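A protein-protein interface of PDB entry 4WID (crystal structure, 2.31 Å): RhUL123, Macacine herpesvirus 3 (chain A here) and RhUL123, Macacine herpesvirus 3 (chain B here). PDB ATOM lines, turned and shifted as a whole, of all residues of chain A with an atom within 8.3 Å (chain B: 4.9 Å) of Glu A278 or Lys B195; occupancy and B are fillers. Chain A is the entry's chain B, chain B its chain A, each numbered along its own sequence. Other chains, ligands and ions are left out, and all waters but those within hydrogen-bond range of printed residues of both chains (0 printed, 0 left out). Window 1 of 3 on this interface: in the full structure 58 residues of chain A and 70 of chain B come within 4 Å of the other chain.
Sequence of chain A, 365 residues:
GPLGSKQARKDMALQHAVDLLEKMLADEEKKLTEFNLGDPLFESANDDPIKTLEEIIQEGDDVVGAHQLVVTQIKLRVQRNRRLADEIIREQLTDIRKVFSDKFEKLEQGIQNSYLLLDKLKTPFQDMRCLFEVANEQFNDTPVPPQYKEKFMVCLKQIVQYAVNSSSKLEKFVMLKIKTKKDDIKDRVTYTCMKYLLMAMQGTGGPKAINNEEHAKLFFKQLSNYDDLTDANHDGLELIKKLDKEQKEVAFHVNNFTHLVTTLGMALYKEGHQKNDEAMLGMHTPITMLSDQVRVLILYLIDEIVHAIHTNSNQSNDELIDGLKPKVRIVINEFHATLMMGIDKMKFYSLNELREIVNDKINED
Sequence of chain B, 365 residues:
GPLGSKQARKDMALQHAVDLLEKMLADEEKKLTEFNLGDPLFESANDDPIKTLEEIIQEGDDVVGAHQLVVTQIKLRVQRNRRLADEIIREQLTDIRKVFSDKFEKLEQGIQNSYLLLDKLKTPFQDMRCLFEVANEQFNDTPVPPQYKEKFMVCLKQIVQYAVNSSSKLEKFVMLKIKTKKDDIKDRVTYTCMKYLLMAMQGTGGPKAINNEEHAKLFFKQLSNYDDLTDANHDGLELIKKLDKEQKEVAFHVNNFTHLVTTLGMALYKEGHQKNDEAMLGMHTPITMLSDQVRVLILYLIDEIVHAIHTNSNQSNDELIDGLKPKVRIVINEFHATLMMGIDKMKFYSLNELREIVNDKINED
The side-chain amino group (NZ) of Lys B195 lies within salt-bridge range of the side-chain carboxylate (OE2) of Glu A278 (2.4 Å). OE1 of Glu A278 sits close to OH of Tyr B196, at 2.3 Å.
Among the printed residues, merely in contact across the chains: Gln A274 with Tyr B196 and Leu A281 with Met B199.
Of chain B, only Lys B195 (2.4 Å) and Tyr B196 (2.3 Å) come within 4 Å of Glu A278. Of chain A, only Glu A278 comes within 4 Å of Lys B195. Of the printed residues of chain A, Tyr B196 touches Gln A274 (3.7 Å) and Glu A278 (2.3 Å). Printed residues of chain B within 4 Å of Leu A281: Met B199 (3.8 Å). Of the printed residues of chain A, Met B199 touches Leu A281. Of the printed residues of chain B, Gln A274 touches Tyr B196. Tyr B191 touches none of the printed residues of chain A. Met A283 touches none of the printed residues of chain B. The nearest printed residue of chain A that does not touch Tyr B196 is Leu A281 (6.6 Å).
Of the 9 printed residues of chain B, 3 touch a printed residue of chain A. Printed residues of chain B that touch a printed residue of chain A: Lys B195, Tyr B196 and Met B199. Printed residues of chain A that touch a printed residue of chain B: Gln A274, Glu A278 and Leu A281. Among the printed residues, Asp or Glu carboxylates within 4 Å of a Lys or Arg side-chain nitrogen of the other chain: Glu A278 with Lys B195.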
ATOM      1  N   SER A 114      32.719  13.628  21.808  1.00  0.00           N
ATOM      2  CA  SER A 114      32.876  14.887  22.541  1.00  0.00           C
ATOM      3  C   SER A 114      33.907  14.796  23.644  1.00  0.00           C
ATOM      4  O   SER A 114      34.581  15.781  23.967  1.00  0.00           O
ATOM      5  CB  SER A 114      31.535  15.326  23.145  1.00  0.00           C
ATOM      6  OG  SER A 114      30.763  15.976  22.175  1.00  0.00           O
ATOM      7  N   LYS A 181      33.080  19.858  32.513  1.00  0.00           N
ATOM      8  CA  LYS A 181      32.261  19.919  31.304  1.00  0.00           C
ATOM      9  C   LYS A 181      32.004  18.542  30.731  1.00  0.00           C
ATOM     10  O   LYS A 181      30.962  18.312  30.147  1.00  0.00           O
ATOM     11  CB  LYS A 181      32.914  20.802  30.246  1.00  0.00           C
ATOM     12  CG  LYS A 181      32.446  22.246  30.296  1.00  0.00           C
ATOM     13  CD  LYS A 181      30.994  22.388  29.860  1.00  0.00           C
ATOM     14  CE  LYS A 181      30.406  23.701  30.369  1.00  0.00           C
ATOM     15  NZ  LYS A 181      31.271  24.850  29.977  1.00  0.00           N
ATOM     16  N   ILE A 185      28.155  16.863  30.356  1.00  0.00           N
ATOM     17  CA  ILE A 185      27.588  16.373  29.107  1.00  0.00           C
ATOM     18  C   ILE A 185      26.860  15.046  29.335  1.00  0.00           C
ATOM     19  O   ILE A 185      25.726  14.870  28.866  1.00  0.00           O
ATOM     20  CB  ILE A 185      28.658  16.225  28.004  1.00  0.00           C
ATOM     21  CG1 ILE A 185      28.954  17.600  27.399  1.00  0.00           C
ATOM     22  CG2 ILE A 185      28.169  15.297  26.914  1.00  0.00           C
ATOM     23  CD1 ILE A 185      30.262  17.691  26.592  1.00  0.00           C
ATOM     24  N   ARG A 188      23.457  15.835  31.169  1.00  0.00           N
ATOM     25  CA  ARG A 188      22.416  16.470  30.379  1.00  0.00           C
ATOM     26  C   ARG A 188      21.833  15.501  29.357  1.00  0.00           C
ATOM     27  O   ARG A 188      20.613  15.376  29.251  1.00  0.00           O
ATOM     28  CB  ARG A 188      22.952  17.729  29.697  1.00  0.00           C
ATOM     29  CG  ARG A 188      23.274  18.829  30.695  1.00  0.00           C
ATOM     30  CD  ARG A 188      24.138  19.932  30.100  1.00  0.00           C
ATOM     31  NE  ARG A 188      24.832  20.667  31.156  1.00  0.00           N
ATOM     32  CZ  ARG A 188      25.542  21.780  30.975  1.00  0.00           C
ATOM     33  NH1 ARG A 188      25.664  22.320  29.765  1.00  0.00           N
ATOM     34  NH2 ARG A 188      26.131  22.358  32.016  1.00  0.00           N
ATOM     35  N   GLU A 271      17.489  16.636  20.597  1.00  0.00           N
ATOM     36  CA  GLU A 271      17.758  17.310  21.860  1.00  0.00           C
ATOM     37  C   GLU A 271      19.096  16.882  22.484  1.00  0.00           C
ATOM     38  O   GLU A 271      19.828  17.725  23.023  1.00  0.00           O
ATOM     39  CB  GLU A 271      16.630  17.089  22.859  1.00  0.00           C
ATOM     40  CG  GLU A 271      16.873  17.844  24.170  1.00  0.00           C
ATOM     41  CD  GLU A 271      15.730  17.680  25.189  1.00  0.00           C
ATOM     42  OE1 GLU A 271      16.034  17.578  26.408  1.00  0.00           O
ATOM     43  OE2 GLU A 271      14.546  17.668  24.759  1.00  0.00           O
ATOM     44  N   GLY A 272      19.413  15.588  22.432  1.00  0.00           N
ATOM     45  CA  GLY A 272      20.648  15.097  23.026  1.00  0.00           C
ATOM     46  C   GLY A 272      21.836  15.734  22.309  1.00  0.00           C
ATOM     47  O   GLY A 272      22.760  16.250  22.931  1.00  0.00           O
ATOM     48  N   HIS A 273      21.764  15.721  20.982  1.00  0.00           N
ATOM     49  CA  HIS A 273      22.741  16.349  20.119  1.00  0.00           C
ATOM     50  C   HIS A 273      22.892  17.841  20.406  1.00  0.00           C
ATOM     51  O   HIS A 273      24.009  18.294  20.657  1.00  0.00           O
ATOM     52  CB  HIS A 273      22.354  16.123  18.660  1.00  0.00           C
ATOM     53  CG  HIS A 273      23.445  16.439  17.690  1.00  0.00           C
ATOM     54  ND1 HIS A 273      23.363  17.485  16.793  1.00  0.00           N
ATOM     55  CD2 HIS A 273      24.645  15.850  17.472  1.00  0.00           C
ATOM     56  CE1 HIS A 273      24.465  17.524  16.066  1.00  0.00           C
ATOM     57  NE2 HIS A 273      25.259  16.543  16.458  1.00  0.00           N
ATOM     58  N   GLN A 274      21.788  18.595  20.362  1.00  0.00           N
ATOM     59  CA  GLN A 274      21.792  20.041  20.646  1.00  0.00           C
ATOM     60  C   GLN A 274      22.413  20.352  22.007  1.00  0.00           C
ATOM     61  O   GLN A 274      23.141  21.337  22.148  1.00  0.00           O
ATOM     62  CB  GLN A 274      20.363  20.626  20.576  1.00  0.00           C
ATOM     63  CG  GLN A 274      20.220  22.164  20.883  1.00  0.00           C
ATOM     64  CD  GLN A 274      18.738  22.652  20.907  1.00  0.00           C
ATOM     65  OE1 GLN A 274      17.865  21.975  21.470  1.00  0.00           O
ATOM     66  NE2 GLN A 274      18.464  23.825  20.306  1.00  0.00           N
ATOM     67  N   LYS A 275      22.143  19.516  23.006  1.00  0.00           N
ATOM     68  CA  LYS A 275      22.726  19.720  24.335  1.00  0.00           C
ATOM     69  C   LYS A 275      24.236  19.493  24.312  1.00  0.00           C
ATOM     70  O   LYS A 275      25.009  20.240  24.929  1.00  0.00           O
ATOM     71  CB  LYS A 275      22.075  18.786  25.366  1.00  0.00           C
ATOM     72  CG  LYS A 275      20.663  19.192  25.801  1.00  0.00           C
ATOM     73  CD  LYS A 275      20.677  20.540  26.509  1.00  0.00           C
ATOM     74  CE  LYS A 275      19.273  21.040  26.803  1.00  0.00           C
ATOM     75  NZ  LYS A 275      19.303  22.474  27.220  1.00  0.00           N
ATOM     76  N   ASN A 276      24.640  18.439  23.610  1.00  0.00           N
ATOM     77  CA  ASN A 276      26.044  18.103  23.420  1.00  0.00           C
ATOM     78  C   ASN A 276      26.816  19.268  22.764  1.00  0.00           C
ATOM     79  O   ASN A 276      27.779  19.780  23.319  1.00  0.00           O
ATOM     80  CB  ASN A 276      26.149  16.821  22.588  1.00  0.00           C
ATOM     81  CG  ASN A 276      27.404  16.040  22.884  1.00  0.00           C
ATOM     82  OD1 ASN A 276      28.478  16.621  22.996  1.00  0.00           O
ATOM     83  ND2 ASN A 276      27.275  14.721  23.037  1.00  0.00           N
ATOM     84  N   ASP A 277      26.351  19.723  21.609  1.00  0.00           N
ATOM     85  CA  ASP A 277      26.987  20.850  20.935  1.00  0.00           C
ATOM     86  C   ASP A 277      27.007  22.171  21.734  1.00  0.00           C
ATOM     87  O   ASP A 277      27.941  22.972  21.569  1.00  0.00           O
ATOM     88  CB  ASP A 277      26.315  21.090  19.583  1.00  0.00           C
ATOM     89  CG  ASP A 277      26.579  19.973  18.591  1.00  0.00           C
ATOM     90  OD1 ASP A 277      27.189  18.955  18.974  1.00  0.00           O
ATOM     91  OD2 ASP A 277      26.155  20.112  17.429  1.00  0.00           O
ATOM     92  N   GLU A 278      25.999  22.418  22.577  1.00  0.00           N
ATOM     93  CA  GLU A 278      25.963  23.667  23.353  1.00  0.00           C
ATOM     94  C   GLU A 278      27.063  23.712  24.416  1.00  0.00           C
ATOM     95  O   GLU A 278      27.616  24.780  24.707  1.00  0.00           O
ATOM     96  CB  GLU A 278      24.606  23.876  24.023  1.00  0.00           C
ATOM     97  CG  GLU A 278      23.606  24.675  23.198  1.00  0.00           C
ATOM     98  CD  GLU A 278      22.292  24.908  23.942  1.00  0.00           C
ATOM     99  OE1 GLU A 278      21.243  25.086  23.277  1.00  0.00           O
ATOM    100  OE2 GLU A 278      22.313  24.917  25.197  1.00  0.00           O
ATOM    101  N   ALA A 279      27.378  22.550  24.979  1.00  0.00           N
ATOM    102  CA  ALA A 279      28.424  22.438  25.988  1.00  0.00           C
ATOM    103  C   ALA A 279      29.808  22.594  25.379  1.00  0.00           C
ATOM    104  O   ALA A 279      30.737  23.079  26.033  1.00  0.00           O
ATOM    105  CB  ALA A 279      28.317  21.110  26.712  1.00  0.00           C
ATOM    106  N   MET A 280      29.947  22.183  24.122  1.00  0.00           N
ATOM    107  CA  MET A 280      31.238  22.269  23.448  1.00  0.00           C
ATOM    108  C   MET A 280      31.512  23.698  23.029  1.00  0.00           C
ATOM    109  O   MET A 280      32.647  24.184  23.141  1.00  0.00           O
ATOM    110  CB  MET A 280      31.272  21.340  22.236  1.00  0.00           C
ATOM    111  CG  MET A 280      31.160  19.868  22.594  1.00  0.00           C
ATOM    112  SD  MET A 280      32.640  19.349  23.470  1.00  0.00           S
ATOM    113  CE  MET A 280      33.937  20.128  22.455  1.00  0.00           C
ATOM    114  N   LEU A 281      30.467  24.366  22.540  1.00  0.00           N
ATOM    115  CA  LEU A 281      30.564  25.753  22.105  1.00  0.00           C
ATOM    116  C   LEU A 281      30.846  26.626  23.298  1.00  0.00           C
ATOM    117  O   LEU A 281      31.588  27.613  23.192  1.00  0.00           O
ATOM    118  CB  LEU A 281      29.299  26.204  21.397  1.00  0.00           C
ATOM    119  CG  LEU A 281      29.330  25.930  19.900  1.00  0.00           C
ATOM    120  CD1 LEU A 281      28.192  26.650  19.217  1.00  0.00           C
ATOM    121  CD2 LEU A 281      30.696  26.364  19.322  1.00  0.00           C
ATOM    122  N   GLY A 282      30.299  26.229  24.446  1.00  0.00           N
ATOM    123  CA  GLY A 282      30.567  26.913  25.699  1.00  0.00           C
ATOM    124  C   GLY A 282      32.034  26.933  26.094  1.00  0.00           C
ATOM    125  O   GLY A 282      32.464  27.808  26.840  1.00  0.00           O
ATOM    126  N   MET A 283      32.803  25.962  25.608  1.00  0.00           N
ATOM    127  CA  MET A 283      34.246  25.902  25.890  1.00  0.00           C
ATOM    128  C   MET A 283      35.070  26.600  24.809  1.00  0.00           C
ATOM    129  O   MET A 283      36.152  27.099  25.077  1.00  0.00           O
ATOM    130  CB  MET A 283      34.712  24.451  26.026  1.00  0.00           C
ATOM    131  CG  MET A 283      34.350  23.804  27.336  1.00  0.00           C
ATOM    132  SD  MET A 283      35.248  24.483  28.745  1.00  0.00           S
ATOM    133  CE  MET A 283      36.908  24.499  28.089  1.00  0.00           C
ATOM    134  N   HIS A 284      34.522  26.633  23.601  1.00  0.00           N
ATOM    135  CA  HIS A 284      35.195  27.115  22.411  1.00  0.00           C
ATOM    136  C   HIS A 284      35.813  28.496  22.585  1.00  0.00           C
ATOM    137  O   HIS A 284      37.036  28.667  22.467  1.00  0.00           O
ATOM    138  CB  HIS A 284      34.208  27.146  21.240  1.00  0.00           C
ATOM    139  CG  HIS A 284      34.837  27.471  19.923  1.00  0.00           C
ATOM    140  ND1 HIS A 284      36.004  26.878  19.486  1.00  0.00           N
ATOM    141  CD2 HIS A 284      34.462  28.326  18.941  1.00  0.00           C
ATOM    142  CE1 HIS A 284      36.317  27.352  18.292  1.00  0.00           C
ATOM    143  NE2 HIS A 284      35.400  28.236  17.940  1.00  0.00           N
ATOM    144  N   TYR B 191      14.126  32.611  23.914  1.00  0.00           N
ATOM    145  CA  TYR B 191      15.201  32.468  24.870  1.00  0.00           C
ATOM    146  C   TYR B 191      16.459  31.923  24.164  1.00  0.00           C
ATOM    147  O   TYR B 191      17.541  32.465  24.323  1.00  0.00           O
ATOM    148  CB  TYR B 191      14.782  31.547  26.014  1.00  0.00           C
ATOM    149  CG  TYR B 191      15.895  31.288  26.987  1.00  0.00           C
ATOM    150  CD1 TYR B 191      16.140  32.159  28.033  1.00  0.00           C
ATOM    151  CD2 TYR B 191      16.724  30.182  26.840  1.00  0.00           C
ATOM    152  CE1 TYR B 191      17.171  31.930  28.926  1.00  0.00           C
ATOM    153  CE2 TYR B 191      17.765  29.951  27.718  1.00  0.00           C
ATOM    154  CZ  TYR B 191      17.979  30.827  28.762  1.00  0.00           C
ATOM    155  OH  TYR B 191      19.012  30.593  29.635  1.00  0.00           O
ATOM    156  N   THR B 192      16.288  30.856  23.393  1.00  0.00           N
ATOM    157  CA  THR B 192      17.355  30.223  22.627  1.00  0.00           C
ATOM    158  C   THR B 192      18.016  31.202  21.666  1.00  0.00           C
ATOM    159  O   THR B 192      19.238  31.300  21.615  1.00  0.00           O
ATOM    160  CB  THR B 192      16.807  29.008  21.859  1.00  0.00           C
ATOM    161  OG1 THR B 192      16.484  27.976  22.799  1.00  0.00           O
ATOM    162  CG2 THR B 192      17.824  28.459  20.882  1.00  0.00           C
ATOM    163  N   CYS B 193      17.194  31.933  20.924  1.00  0.00           N
ATOM    164  CA  CYS B 193      17.636  33.035  20.079  1.00  0.00           C
ATOM    165  C   CYS B 193      18.530  34.038  20.821  1.00  0.00           C
ATOM    166  O   CYS B 193      19.602  34.415  20.336  1.00  0.00           O
ATOM    167  CB  CYS B 193      16.414  33.758  19.498  1.00  0.00           C
ATOM    168  SG  CYS B 193      15.711  32.909  18.066  1.00  0.00           S
ATOM    169  N   MET B 194      18.091  34.472  21.997  1.00  0.00           N
ATOM    170  CA  MET B 194      18.866  35.423  22.762  1.00  0.00           C
ATOM    171  C   MET B 194      20.161  34.814  23.308  1.00  0.00           C
ATOM    172  O   MET B 194      21.173  35.485  23.426  1.00  0.00           O
ATOM    173  CB  MET B 194      18.028  35.978  23.899  1.00  0.00           C
ATOM    174  CG  MET B 194      16.772  36.672  23.392  1.00  0.00           C
ATOM    175  SD  MET B 194      15.882  37.573  24.676  1.00  0.00           S
ATOM    176  CE  MET B 194      16.171  36.500  26.086  1.00  0.00           C
ATOM    177  N   LYS B 195      20.099  33.548  23.674  1.00  0.00           N
ATOM    178  CA  LYS B 195      21.235  32.875  24.246  1.00  0.00           C
ATOM    179  C   LYS B 195      22.341  32.753  23.176  1.00  0.00           C
ATOM    180  O   LYS B 195      23.500  33.004  23.431  1.00  0.00           O
ATOM    181  CB  LYS B 195      20.805  31.501  24.770  1.00  0.00           C
ATOM    182  CG  LYS B 195      21.877  30.796  25.578  1.00  0.00           C
ATOM    183  CD  LYS B 195      21.724  29.281  25.489  1.00  0.00           C
ATOM    184  CE  LYS B 195      22.898  28.582  26.166  1.00  0.00           C
ATOM    185  NZ  LYS B 195      22.763  27.097  26.110  1.00  0.00           N
ATOM    186  N   TYR B 196      21.963  32.381  21.966  1.00  0.00           N
ATOM    187  CA  TYR B 196      22.958  32.116  20.948  1.00  0.00           C
ATOM    188  C   TYR B 196      23.552  33.441  20.489  1.00  0.00           C
ATOM    189  O   TYR B 196      24.748  33.541  20.171  1.00  0.00           O
ATOM    190  CB  TYR B 196      22.341  31.338  19.797  1.00  0.00           C
ATOM    191  CG  TYR B 196      22.090  29.884  20.158  1.00  0.00           C
ATOM    192  CD1 TYR B 196      22.482  29.379  21.386  1.00  0.00           C
ATOM    193  CD2 TYR B 196      21.474  29.015  19.265  1.00  0.00           C
ATOM    194  CE1 TYR B 196      22.263  28.061  21.725  1.00  0.00           C
ATOM    195  CE2 TYR B 196      21.256  27.695  19.591  1.00  0.00           C
ATOM    196  CZ  TYR B 196      21.651  27.224  20.827  1.00  0.00           C
ATOM    197  OH  TYR B 196      21.429  25.901  21.161  1.00  0.00           O
ATOM    198  N   LEU B 197      22.714  34.466  20.515  1.00  0.00           N
ATOM    199  CA  LEU B 197      23.144  35.797  20.150  1.00  0.00           C
ATOM    200  C   LEU B 197      24.226  36.309  21.104  1.00  0.00           C
ATOM    201  O   LEU B 197      25.200  36.944  20.670  1.00  0.00           O
ATOM    202  CB  LEU B 197      21.946  36.744  20.124  1.00  0.00           C
ATOM    203  CG  LEU B 197      22.248  38.196  19.792  1.00  0.00           C
ATOM    204  CD1 LEU B 197      23.115  38.293  18.521  1.00  0.00           C
ATOM    205  CD2 LEU B 197      20.941  38.913  19.613  1.00  0.00           C
ATOM    206  N   LEU B 198      24.061  36.040  22.397  1.00  0.00           N
ATOM    207  CA  LEU B 198      25.056  36.483  23.374  1.00  0.00           C
ATOM    208  C   LEU B 198      26.398  35.782  23.157  1.00  0.00           C
ATOM    209  O   LEU B 198      27.454  36.418  23.140  1.00  0.00           O
ATOM    210  CB  LEU B 198      24.557  36.247  24.790  1.00  0.00           C
ATOM    211  CG  LEU B 198      23.428  37.210  25.129  1.00  0.00           C
ATOM    212  CD1 LEU B 198      22.407  36.599  26.096  1.00  0.00           C
ATOM    213  CD2 LEU B 198      24.032  38.494  25.689  1.00  0.00           C
ATOM    214  N   MET B 199      26.331  34.467  22.992  1.00  0.00           N
ATOM    215  CA  MET B 199      27.487  33.623  22.741  1.00  0.00           C
ATOM    216  C   MET B 199      28.225  34.049  21.470  1.00  0.00           C
ATOM    217  O   MET B 199      29.441  33.887  21.363  1.00  0.00           O
ATOM    218  CB  MET B 199      27.043  32.156  22.640  1.00  0.00           C
ATOM    219  CG  MET B 199      26.533  31.555  23.954  1.00  0.00           C
ATOM    220  SD  MET B 199      26.020  29.829  23.762  1.00  0.00           S
ATOM    221  CE  MET B 199      27.480  29.090  23.023  1.00  0.00           C
